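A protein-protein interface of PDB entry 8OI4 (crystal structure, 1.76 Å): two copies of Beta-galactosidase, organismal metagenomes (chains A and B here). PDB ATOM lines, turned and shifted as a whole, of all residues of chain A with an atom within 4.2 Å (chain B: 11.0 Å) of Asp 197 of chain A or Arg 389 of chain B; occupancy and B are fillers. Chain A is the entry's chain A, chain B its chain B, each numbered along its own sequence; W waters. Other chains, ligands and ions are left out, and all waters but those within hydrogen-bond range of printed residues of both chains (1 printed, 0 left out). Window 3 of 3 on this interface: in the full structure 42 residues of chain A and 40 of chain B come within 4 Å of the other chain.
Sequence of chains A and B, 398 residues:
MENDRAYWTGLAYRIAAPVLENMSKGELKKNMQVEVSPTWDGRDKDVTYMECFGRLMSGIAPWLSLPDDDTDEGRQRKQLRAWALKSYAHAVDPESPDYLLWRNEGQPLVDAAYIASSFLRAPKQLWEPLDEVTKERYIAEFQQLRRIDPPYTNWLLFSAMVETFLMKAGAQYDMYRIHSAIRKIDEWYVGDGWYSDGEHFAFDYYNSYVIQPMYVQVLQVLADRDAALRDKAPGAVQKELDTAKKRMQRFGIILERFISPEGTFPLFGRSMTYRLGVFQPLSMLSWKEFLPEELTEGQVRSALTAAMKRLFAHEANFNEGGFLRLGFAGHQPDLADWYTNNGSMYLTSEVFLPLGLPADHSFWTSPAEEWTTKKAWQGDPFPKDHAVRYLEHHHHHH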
ATOM      1  N   THR A 153      21.929  -4.698  26.153  1.00  0.00           N
ATOM      2  CA  THR A 153      20.935  -5.629  25.659  1.00  0.00           C
ATOM      3  C   THR A 153      19.883  -4.807  24.932  1.00  0.00           C
ATOM      4  O   THR A 153      20.086  -3.628  24.629  1.00  0.00           O
ATOM      5  CB  THR A 153      20.301  -6.431  26.821  1.00  0.00           C
ATOM      6  OG1 THR A 153      19.552  -5.518  27.624  1.00  0.00           O
ATOM      7  CG2 THR A 153      21.316  -7.167  27.655  1.00  0.00           C
ATOM      8  N   ASN A 154      18.724  -5.431  24.719  1.00  0.00           N
ATOM      9  CA  ASN A 154      17.561  -4.720  24.212  1.00  0.00           C
ATOM     10  C   ASN A 154      17.248  -3.433  24.988  1.00  0.00           C
ATOM     11  O   ASN A 154      16.614  -2.532  24.444  1.00  0.00           O
ATOM     12  CB  ASN A 154      16.359  -5.659  24.213  1.00  0.00           C
ATOM     13  CG  ASN A 154      15.815  -5.926  25.586  1.00  0.00           C
ATOM     14  OD1 ASN A 154      15.030  -5.145  26.107  1.00  0.00           O
ATOM     15  ND2 ASN A 154      16.192  -7.043  26.179  1.00  0.00           N
ATOM     16  N   TYR A 195      17.509 -10.994  15.421  1.00  0.00           N
ATOM     17  CA  TYR A 195      18.537 -10.253  16.125  1.00  0.00           C
ATOM     18  C   TYR A 195      18.932 -10.941  17.429  1.00  0.00           C
ATOM     19  O   TYR A 195      18.114 -11.662  18.009  1.00  0.00           O
ATOM     20  CB  TYR A 195      18.014  -8.886  16.533  1.00  0.00           C
ATOM     21  CG  TYR A 195      17.693  -7.935  15.418  1.00  0.00           C
ATOM     22  CD1 TYR A 195      16.530  -8.071  14.669  1.00  0.00           C
ATOM     23  CD2 TYR A 195      18.523  -6.865  15.138  1.00  0.00           C
ATOM     24  CE1 TYR A 195      16.216  -7.179  13.667  1.00  0.00           C
ATOM     25  CE2 TYR A 195      18.211  -5.950  14.143  1.00  0.00           C
ATOM     26  CZ  TYR A 195      17.051  -6.095  13.422  1.00  0.00           C
ATOM     27  OH  TYR A 195      16.727  -5.177  12.466  1.00  0.00           O
ATOM     28  N   SER A 196      20.166 -10.686  17.894  1.00  0.00           N
ATOM     29  CA  SER A 196      20.592 -11.094  19.225  1.00  0.00           C
ATOM     30  C   SER A 196      20.179 -10.032  20.243  1.00  0.00           C
ATOM     31  O   SER A 196      20.227  -8.837  19.969  1.00  0.00           O
ATOM     32  CB  SER A 196      22.090 -11.372  19.312  1.00  0.00           C
ATOM     33  OG  SER A 196      22.822 -10.226  18.909  1.00  0.00           O
ATOM     34  N   ASP A 197      19.766 -10.503  21.417  1.00  0.00           N
ATOM     35  CA  ASP A 197      19.426  -9.648  22.543  1.00  0.00           C
ATOM     36  C   ASP A 197      20.710  -9.351  23.310  1.00  0.00           C
ATOM     37  O   ASP A 197      20.992  -9.935  24.350  1.00  0.00           O
ATOM     38  CB  ASP A 197      18.380 -10.335  23.426  1.00  0.00           C
ATOM     39  CG  ASP A 197      17.947  -9.476  24.615  1.00  0.00           C
ATOM     40  OD1 ASP A 197      18.183  -8.249  24.578  1.00  0.00           O
ATOM     41  OD2 ASP A 197      17.440 -10.044  25.599  1.00  0.00           O
ATOM     42  N   GLY A 198      21.506  -8.435  22.766  1.00  0.00           N
ATOM     43  CA  GLY A 198      22.846  -8.209  23.252  1.00  0.00           C
ATOM     44  C   GLY A 198      23.875  -9.012  22.466  1.00  0.00           C
ATOM     45  O   GLY A 198      23.605  -9.465  21.360  1.00  0.00           O
ATOM     46  N   HIS A 200      25.193 -11.905  22.832  1.00  0.00           N
ATOM     47  CA  HIS A 200      24.991 -13.338  22.708  1.00  0.00           C
ATOM     48  C   HIS A 200      23.563 -13.596  22.234  1.00  0.00           C
ATOM     49  O   HIS A 200      22.602 -13.028  22.750  1.00  0.00           O
ATOM     50  CB  HIS A 200      25.387 -14.026  24.022  1.00  0.00           C
ATOM     51  CG  HIS A 200      26.864 -13.980  24.310  1.00  0.00           C
ATOM     52  ND1 HIS A 200      27.429 -13.139  25.244  1.00  0.00           N
ATOM     53  CD2 HIS A 200      27.897 -14.634  23.749  1.00  0.00           C
ATOM     54  CE1 HIS A 200      28.748 -13.313  25.263  1.00  0.00           C
ATOM     55  NE2 HIS A 200      29.058 -14.219  24.361  1.00  0.00           N
ATOM     56  N   ALA A 202      20.063 -15.213  21.900  1.00  0.00           N
ATOM     57  CA  ALA A 202      19.135 -15.964  22.721  1.00  0.00           C
ATOM     58  C   ALA A 202      17.935 -16.281  21.843  1.00  0.00           C
ATOM     59  O   ALA A 202      17.406 -15.418  21.148  1.00  0.00           O
ATOM     60  CB  ALA A 202      18.707 -15.158  23.950  1.00  0.00           C
ATOM     61  N   TYR A 206      12.133 -11.814  22.609  1.00  0.00           N
ATOM     62  CA  TYR A 206      12.493 -10.414  22.795  1.00  0.00           C
ATOM     63  C   TYR A 206      12.615  -9.660  21.474  1.00  0.00           C
ATOM     64  O   TYR A 206      12.434  -8.442  21.449  1.00  0.00           O
ATOM     65  CB  TYR A 206      13.713 -10.223  23.723  1.00  0.00           C
ATOM     66  CG  TYR A 206      13.240 -10.129  25.151  1.00  0.00           C
ATOM     67  CD1 TYR A 206      13.005 -11.272  25.905  1.00  0.00           C
ATOM     68  CD2 TYR A 206      12.889  -8.908  25.704  1.00  0.00           C
ATOM     69  CE1 TYR A 206      12.506 -11.191  27.206  1.00  0.00           C
ATOM     70  CE2 TYR A 206      12.389  -8.818  26.993  1.00  0.00           C
ATOM     71  CZ  TYR A 206      12.193  -9.963  27.744  1.00  0.00           C
ATOM     72  OH  TYR A 206      11.679  -9.861  29.022  1.00  0.00           O
ATOM     73  N   ILE A 211      12.773  -5.644  20.474  1.00  0.00           N
ATOM     74  CA  ILE A 211      13.829  -5.239  19.573  1.00  0.00           C
ATOM     75  C   ILE A 211      13.292  -4.678  18.260  1.00  0.00           C
ATOM     76  O   ILE A 211      13.594  -3.546  17.909  1.00  0.00           O
ATOM     77  CB  ILE A 211      14.851  -6.362  19.347  1.00  0.00           C
ATOM     78  CG1 ILE A 211      15.505  -6.750  20.684  1.00  0.00           C
ATOM     79  CG2 ILE A 211      15.905  -5.954  18.269  1.00  0.00           C
ATOM     80  CD1 ILE A 211      16.325  -8.041  20.598  1.00  0.00           C
ATOM     81  N   ARG A 270      12.844 -16.822  27.772  1.00  0.00           N
ATOM     82  CA  ARG A 270      12.351 -16.231  29.007  1.00  0.00           C
ATOM     83  C   ARG A 270      11.145 -15.333  28.728  1.00  0.00           C
ATOM     84  O   ARG A 270      10.843 -14.979  27.574  1.00  0.00           O
ATOM     85  CB  ARG A 270      13.485 -15.471  29.706  1.00  0.00           C
ATOM     86  CG  ARG A 270      13.945 -14.270  28.923  1.00  0.00           C
ATOM     87  CD  ARG A 270      15.225 -13.665  29.491  1.00  0.00           C
ATOM     88  NE  ARG A 270      15.646 -12.542  28.654  1.00  0.00           N
ATOM     89  CZ  ARG A 270      15.367 -11.272  28.919  1.00  0.00           C
ATOM     90  NH1 ARG A 270      14.653 -10.930  29.988  1.00  0.00           N
ATOM     91  NH2 ARG A 270      15.790 -10.328  28.083  1.00  0.00           N
ATOM     92  N   TYR B 189      28.475 -21.729  14.675  1.00  0.00           N
ATOM     93  CA  TYR B 189      27.572 -21.731  15.813  1.00  0.00           C
ATOM     94  C   TYR B 189      27.178 -20.292  16.123  1.00  0.00           C
ATOM     95  O   TYR B 189      28.025 -19.435  16.277  1.00  0.00           O
ATOM     96  CB  TYR B 189      28.215 -22.370  17.015  1.00  0.00           C
ATOM     97  CG  TYR B 189      27.294 -22.452  18.205  1.00  0.00           C
ATOM     98  CD1 TYR B 189      26.130 -23.204  18.154  1.00  0.00           C
ATOM     99  CD2 TYR B 189      27.580 -21.774  19.372  1.00  0.00           C
ATOM    100  CE1 TYR B 189      25.280 -23.302  19.258  1.00  0.00           C
ATOM    101  CE2 TYR B 189      26.739 -21.852  20.474  1.00  0.00           C
ATOM    102  CZ  TYR B 189      25.590 -22.622  20.414  1.00  0.00           C
ATOM    103  OH  TYR B 189      24.770 -22.680  21.516  1.00  0.00           O
ATOM    104  N   VAL B 190      25.876 -20.036  16.171  1.00  0.00           N
ATOM    105  CA  VAL B 190      25.362 -18.696  16.396  1.00  0.00           C
ATOM    106  C   VAL B 190      25.106 -18.484  17.883  1.00  0.00           C
ATOM    107  O   VAL B 190      25.484 -17.472  18.461  1.00  0.00           O
ATOM    108  CB  VAL B 190      24.075 -18.454  15.573  1.00  0.00           C
ATOM    109  CG1 VAL B 190      23.388 -17.191  16.018  1.00  0.00           C
ATOM    110  CG2 VAL B 190      24.399 -18.393  14.076  1.00  0.00           C
ATOM    111  N   GLY B 191      24.478 -19.455  18.519  1.00  0.00           N
ATOM    112  CA  GLY B 191      24.214 -19.345  19.944  1.00  0.00           C
ATOM    113  C   GLY B 191      22.881 -19.995  20.277  1.00  0.00           C
ATOM    114  O   GLY B 191      22.067 -20.267  19.408  1.00  0.00           O
ATOM    115  N   ASP B 192      22.692 -20.210  21.570  1.00  0.00           N
ATOM    116  CA  ASP B 192      21.495 -20.802  22.133  1.00  0.00           C
ATOM    117  C   ASP B 192      20.956 -21.992  21.343  1.00  0.00           C
ATOM    118  O   ASP B 192      19.753 -22.102  21.102  1.00  0.00           O
ATOM    119  CB  ASP B 192      20.422 -19.732  22.345  1.00  0.00           C
ATOM    120  CG  ASP B 192      19.429 -20.138  23.428  1.00  0.00           C
ATOM    121  OD1 ASP B 192      19.746 -21.079  24.203  1.00  0.00           O
ATOM    122  OD2 ASP B 192      18.356 -19.511  23.514  1.00  0.00           O
ATOM    123  N   GLY B 193      21.882 -22.888  20.965  1.00  0.00           N
ATOM    124  CA  GLY B 193      21.552 -24.127  20.287  1.00  0.00           C
ATOM    125  C   GLY B 193      21.511 -24.093  18.762  1.00  0.00           C
ATOM    126  O   GLY B 193      21.276 -25.124  18.147  1.00  0.00           O
ATOM    127  N   TRP B 194      21.710 -22.913  18.165  1.00  0.00           N
ATOM    128  CA  TRP B 194      21.541 -22.735  16.726  1.00  0.00           C
ATOM    129  C   TRP B 194      22.858 -22.516  15.989  1.00  0.00           C
ATOM    130  O   TRP B 194      23.712 -21.765  16.455  1.00  0.00           O
ATOM    131  CB  TRP B 194      20.632 -21.528  16.452  1.00  0.00           C
ATOM    132  CG  TRP B 194      19.192 -21.779  16.706  1.00  0.00           C
ATOM    133  CD1 TRP B 194      18.503 -21.543  17.864  1.00  0.00           C
ATOM    134  CD2 TRP B 194      18.245 -22.257  15.763  1.00  0.00           C
ATOM    135  NE1 TRP B 194      17.186 -21.905  17.702  1.00  0.00           N
ATOM    136  CE2 TRP B 194      17.000 -22.336  16.416  1.00  0.00           C
ATOM    137  CE3 TRP B 194      18.324 -22.645  14.419  1.00  0.00           C
ATOM    138  CZ2 TRP B 194      15.847 -22.778  15.763  1.00  0.00           C
ATOM    139  CZ3 TRP B 194      17.185 -23.104  13.785  1.00  0.00           C
ATOM    140  CH2 TRP B 194      15.967 -23.152  14.452  1.00  0.00           C
ATOM    141  N   THR B 243      30.893 -30.046  24.005  1.00  0.00           N
ATOM    142  CA  THR B 243      30.195 -28.836  23.603  1.00  0.00           C
ATOM    143  C   THR B 243      29.137 -29.097  22.537  1.00  0.00           C
ATOM    144  O   THR B 243      28.030 -28.579  22.618  1.00  0.00           O
ATOM    145  CB  THR B 243      31.220 -27.794  23.140  1.00  0.00           C
ATOM    146  OG1 THR B 243      32.065 -27.507  24.241  1.00  0.00           O
ATOM    147  CG2 THR B 243      30.561 -26.499  22.639  1.00  0.00           C
ATOM    148  N   LYS B 246      26.126 -30.685  24.169  1.00  0.00           N
ATOM    149  CA  LYS B 246      25.374 -29.712  24.947  1.00  0.00           C
ATOM    150  C   LYS B 246      24.560 -28.778  24.058  1.00  0.00           C
ATOM    151  O   LYS B 246      23.427 -28.435  24.384  1.00  0.00           O
ATOM    152  CB  LYS B 246      26.283 -28.877  25.831  1.00  0.00           C
ATOM    153  CG  LYS B 246      26.829 -29.629  27.043  1.00  0.00           C
ATOM    154  CD  LYS B 246      27.764 -28.695  27.834  1.00  0.00           C
ATOM    155  CE  LYS B 246      28.692 -29.428  28.779  1.00  0.00           C
ATOM    156  NZ  LYS B 246      27.941 -30.366  29.637  1.00  0.00           N
ATOM    157  N   ARG B 247      25.142 -28.364  22.931  1.00  0.00           N
ATOM    158  CA  ARG B 247      24.416 -27.549  21.979  1.00  0.00           C
ATOM    159  C   ARG B 247      23.220 -28.313  21.424  1.00  0.00           C
ATOM    160  O   ARG B 247      22.132 -27.748  21.291  1.00  0.00           O
ATOM    161  CB  ARG B 247      25.312 -27.094  20.836  1.00  0.00           C
ATOM    162  CG  ARG B 247      26.371 -26.107  21.247  1.00  0.00           C
ATOM    163  CD  ARG B 247      27.354 -25.968  20.141  1.00  0.00           C
ATOM    164  NE  ARG B 247      28.417 -25.007  20.407  1.00  0.00           N
ATOM    165  CZ  ARG B 247      29.478 -24.873  19.630  1.00  0.00           C
ATOM    166  NH1 ARG B 247      29.651 -25.629  18.554  1.00  0.00           N
ATOM    167  NH2 ARG B 247      30.399 -23.984  19.958  1.00  0.00           N
ATOM    168  N   ARG B 250      20.353 -28.502  23.883  1.00  0.00           N
ATOM    169  CA  ARG B 250      19.563 -27.282  23.868  1.00  0.00           C
ATOM    170  C   ARG B 250      18.633 -27.239  22.660  1.00  0.00           C
ATOM    171  O   ARG B 250      17.463 -26.887  22.778  1.00  0.00           O
ATOM    172  CB  ARG B 250      20.475 -26.058  23.919  1.00  0.00           C
ATOM    173  CG  ARG B 250      19.725 -24.742  23.738  1.00  0.00           C
ATOM    174  CD  ARG B 250      18.702 -24.530  24.816  1.00  0.00           C
ATOM    175  NE  ARG B 250      18.073 -23.212  24.701  1.00  0.00           N
ATOM    176  CZ  ARG B 250      16.812 -22.940  25.027  1.00  0.00           C
ATOM    177  NH1 ARG B 250      16.046 -23.831  25.632  1.00  0.00           N
ATOM    178  NH2 ARG B 250      16.315 -21.737  24.745  1.00  0.00           N
ATOM    179  N   PHE B 251      19.151 -27.610  21.483  1.00  0.00           N
ATOM    180  CA  PHE B 251      18.327 -27.631  20.293  1.00  0.00           C
ATOM    181  C   PHE B 251      17.169 -28.632  20.449  1.00  0.00           C
ATOM    182  O   PHE B 251      16.059 -28.373  20.000  1.00  0.00           O
ATOM    183  CB  PHE B 251      19.169 -27.947  19.061  1.00  0.00           C
ATOM    184  CG  PHE B 251      18.448 -27.622  17.781  1.00  0.00           C
ATOM    185  CD1 PHE B 251      18.186 -26.302  17.429  1.00  0.00           C
ATOM    186  CD2 PHE B 251      18.012 -28.625  16.935  1.00  0.00           C
ATOM    187  CE1 PHE B 251      17.504 -26.004  16.255  1.00  0.00           C
ATOM    188  CE2 PHE B 251      17.331 -28.325  15.767  1.00  0.00           C
ATOM    189  CZ  PHE B 251      17.074 -27.021  15.427  1.00  0.00           C
ATOM    190  N   ILE B 254      14.455 -27.030  22.413  1.00  0.00           N
ATOM    191  CA  ILE B 254      13.729 -26.154  21.509  1.00  0.00           C
ATOM    192  C   ILE B 254      12.762 -26.947  20.631  1.00  0.00           C
ATOM    193  O   ILE B 254      11.592 -26.582  20.507  1.00  0.00           O
ATOM    194  CB  ILE B 254      14.727 -25.298  20.680  1.00  0.00           C
ATOM    195  CG1 ILE B 254      15.471 -24.305  21.584  1.00  0.00           C
ATOM    196  CG2 ILE B 254      14.026 -24.604  19.507  1.00  0.00           C
ATOM    197  CD1 ILE B 254      16.661 -23.702  20.953  1.00  0.00           C
ATOM    198  N   ASP B 385      11.791 -21.570  30.465  1.00  0.00           N
ATOM    199  CA  ASP B 385      12.895 -21.900  29.573  1.00  0.00           C
ATOM    200  C   ASP B 385      14.014 -20.885  29.780  1.00  0.00           C
ATOM    201  O   ASP B 385      13.761 -19.741  30.158  1.00  0.00           O
ATOM    202  CB  ASP B 385      12.421 -21.894  28.128  1.00  0.00           C
ATOM    203  CG  ASP B 385      13.411 -22.470  27.122  1.00  0.00           C
ATOM    204  OD1 ASP B 385      14.043 -23.532  27.439  1.00  0.00           O
ATOM    205  OD2 ASP B 385      13.557 -21.867  26.010  1.00  0.00           O
ATOM    206  N   HIS B 386      15.255 -21.326  29.553  1.00  0.00           N
ATOM    207  CA  HIS B 386      16.421 -20.488  29.795  1.00  0.00           C
ATOM    208  C   HIS B 386      17.364 -20.628  28.608  1.00  0.00           C
ATOM    209  O   HIS B 386      17.545 -21.728  28.113  1.00  0.00           O
ATOM    210  CB  HIS B 386      17.123 -20.908  31.093  1.00  0.00           C
ATOM    211  CG  HIS B 386      16.282 -20.812  32.331  1.00  0.00           C
ATOM    212  ND1 HIS B 386      15.706 -21.909  32.943  1.00  0.00           N
ATOM    213  CD2 HIS B 386      15.926 -19.743  33.083  1.00  0.00           C
ATOM    214  CE1 HIS B 386      15.022 -21.509  34.013  1.00  0.00           C
ATOM    215  NE2 HIS B 386      15.135 -20.195  34.111  1.00  0.00           N
ATOM    216  N   ALA B 387      17.914 -19.503  28.152  1.00  0.00           N
ATOM    217  CA  ALA B 387      18.940 -19.511  27.121  1.00  0.00           C
ATOM    218  C   ALA B 387      20.188 -20.181  27.688  1.00  0.00           C
ATOM    219  O   ALA B 387      20.468 -20.063  28.882  1.00  0.00           O
ATOM    220  CB  ALA B 387      19.271 -18.101  26.676  1.00  0.00           C
ATOM    221  N   VAL B 388      20.931 -20.854  26.817  1.00  0.00           N
ATOM    222  CA  VAL B 388      22.255 -21.333  27.153  1.00  0.00           C
ATOM    223  C   VAL B 388      23.210 -20.502  26.302  1.00  0.00           C
ATOM    224  O   VAL B 388      23.280 -20.675  25.095  1.00  0.00           O
ATOM    225  CB  VAL B 388      22.397 -22.862  26.960  1.00  0.00           C
ATOM    226  CG1 VAL B 388      21.319 -23.615  27.718  1.00  0.00           C
ATOM    227  CG2 VAL B 388      22.396 -23.242  25.496  1.00  0.00           C
ATOM    228  N   ARG B 389      23.905 -19.556  26.930  1.00  0.00           N
ATOM    229  CA  ARG B 389      24.646 -18.529  26.209  1.00  0.00           C
ATOM    230  C   ARG B 389      26.157 -18.761  26.260  1.00  0.00           C
ATOM    231  O   ARG B 389      26.917 -17.962  25.730  1.00  0.00           O
ATOM    232  CB  ARG B 389      24.293 -17.119  26.761  1.00  0.00           C
ATOM    233  CG  ARG B 389      22.848 -16.700  26.403  1.00  0.00           C
ATOM    234  CD  ARG B 389      22.311 -15.494  27.174  1.00  0.00           C
ATOM    235  NE  ARG B 389      22.271 -14.281  26.362  1.00  0.00           N
ATOM    236  CZ  ARG B 389      21.185 -13.550  26.135  1.00  0.00           C
ATOM    237  NH1 ARG B 389      20.123 -13.618  26.930  1.00  0.00           N
ATOM    238  NH2 ARG B 389      21.165 -12.729  25.086  1.00  0.00           N
ATOM    239  N   TYR B 390      26.582 -19.867  26.878  1.00  0.00           N
ATOM    240  CA  TYR B 390      27.971 -20.095  27.259  1.00  0.00           C
ATOM    241  C   TYR B 390      28.689 -21.167  26.433  1.00  0.00           C
ATOM    242  O   TYR B 390      29.772 -21.612  26.813  1.00  0.00           O
ATOM    243  CB  TYR B 390      28.057 -20.481  28.775  1.00  0.00           C
ATOM    244  CG  TYR B 390      27.001 -21.462  29.261  1.00  0.00           C
ATOM    245  CD1 TYR B 390      25.763 -21.017  29.706  1.00  0.00           C
ATOM    246  CD2 TYR B 390      27.240 -22.836  29.266  1.00  0.00           C
ATOM    247  CE1 TYR B 390      24.795 -21.904  30.165  1.00  0.00           C
ATOM    248  CE2 TYR B 390      26.268 -23.736  29.697  1.00  0.00           C
ATOM    249  CZ  TYR B 390      25.041 -23.265  30.140  1.00  0.00           C
ATOM    250  OH  TYR B 390      24.053 -24.123  30.564  1.00  0.00           O
ATOM    251  N   LEU B 391      28.107 -21.567  25.295  1.00  0.00           N
ATOM    252  CA  LEU B 391      28.655 -22.671  24.514  1.00  0.00           C
ATOM    253  C   LEU B 391      29.393 -22.192  23.240  1.00  0.00           C
ATOM    254  O   LEU B 391      29.633 -22.998  22.363  1.00  0.00           O
ATOM    255  CB  LEU B 391      27.522 -23.645  24.137  1.00  0.00           C
ATOM    256  CG  LEU B 391      26.714 -24.224  25.317  1.00  0.00           C
ATOM    257  CD1 LEU B 391      25.537 -25.046  24.830  1.00  0.00           C
ATOM    258  CD2 LEU B 391      27.608 -25.045  26.239  1.00  0.00           C
HETATM  259  O   HOH W   1      17.078 -12.535  25.938  1.00  0.00           O
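The guanidinium group (NH2) of Arg 389 of chain B sits at hydrogen-bond distance from the backbone carbonyl oxygen (O) of Asp 197 of chain A, at 2.9 Å. The guanidinium group (NH2) of Arg 389 of chain B lies within hydrogen-bond range of the backbone carbonyl oxygen (O) of His 200 of chain A.
The guanidinium group (NH2) of Arg 270 of chain A is in salt-bridge range of the side-chain carboxylate (OD2) of Asp 197 of chain A (3.0 Å). OH of Tyr 206 of chain A sits at hydrogen-bond distance from NH1 of Arg 270 of chain A. The side-chain hydroxyl (OH) of Tyr 189 of chain B is in hydrogen-bond range of the backbone NH (N) of Asp 192 of chain B (3.2 Å). The side-chain carboxylate (OD1) of Asp 192 of chain B is in salt-bridge range of the guanidinium group (NE) of Arg 250 of chain B. The backbone NH (N) of Val 388 of chain B sits at hydrogen-bond distance from the side-chain carboxylate (OD1) of Asp 192 of chain B. NH1 of Arg 250 of chain B is in salt-bridge range of OD1 of Asp 385 of chain B (2.7 Å).
Ala 202 of chain A touches Asp 192 of chain B (C to OD2, 3.7 Å). NH2 of Arg 389 of chain B touches CB of Ala 202 of chain A (3.6 Å). Arg 270 of chain A touches Asp 385 of chain B (N to O, 3.9 Å).
Of chain B, only Arg 389 comes within 4 Å of Asp 197 of chain A. Arg 389 of chain B touches just these residues of chain A: Asp 197 (2.9 Å), His 200 (2.8 Å) and Ala 202 (3.6 Å). Asn 154 of chain A touches none of the printed residues of chain B. No residue of chain B comes within 4 Å of Gly 198 of chain A. His 200 of chain A touches one residue of chain B. Of the printed residues of chain A, Asp 385 of chain B touches Arg 270 (3.9 Å). Of the printed residues of chain A, Asp 192 of chain B touches Ala 202 (3.7 Å). Of the printed residues of chain B, Arg 270 of chain A touches Asp 385 (3.9 Å). Leu 391 of chain B touches none of the printed residues of chain A. Lys 246 of chain B touches none of the printed residues of chain A. The nearest residue of chain B that does not touch Asp 197 of chain A is Ala 387 of chain B (8.3 Å). The nearest printed residue of chain A that does not touch Arg 389 of chain B is Gly 198 of chain A (4.9 Å). The nearest printed residue of chain A that does not touch Asp 192 of chain B is His 200 of chain A (6.7 Å).
Of the 11 printed residues of chain A, 4 touch a printed residue of chain B. Of the 19 printed residues of chain B, 3 touch a printed residue of chain A. Along chain B the printed residues that touch a printed residue of chain A span positions 192 to 389. Among the printed residues, 5 pairs touch across the chains.
No position is printed for both chains. Of the 5 pairs that touch across the chains among the printed residues, none has its exchanged pair printed and touching as well.
Water W1 lies within hydrogen-bond range of OD2 of Asp 197 of chain A (2.5 Å), NE of Arg 270 of chain A (3.1 Å) and NH1 of Arg 389 of chain B (3.4 Å).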
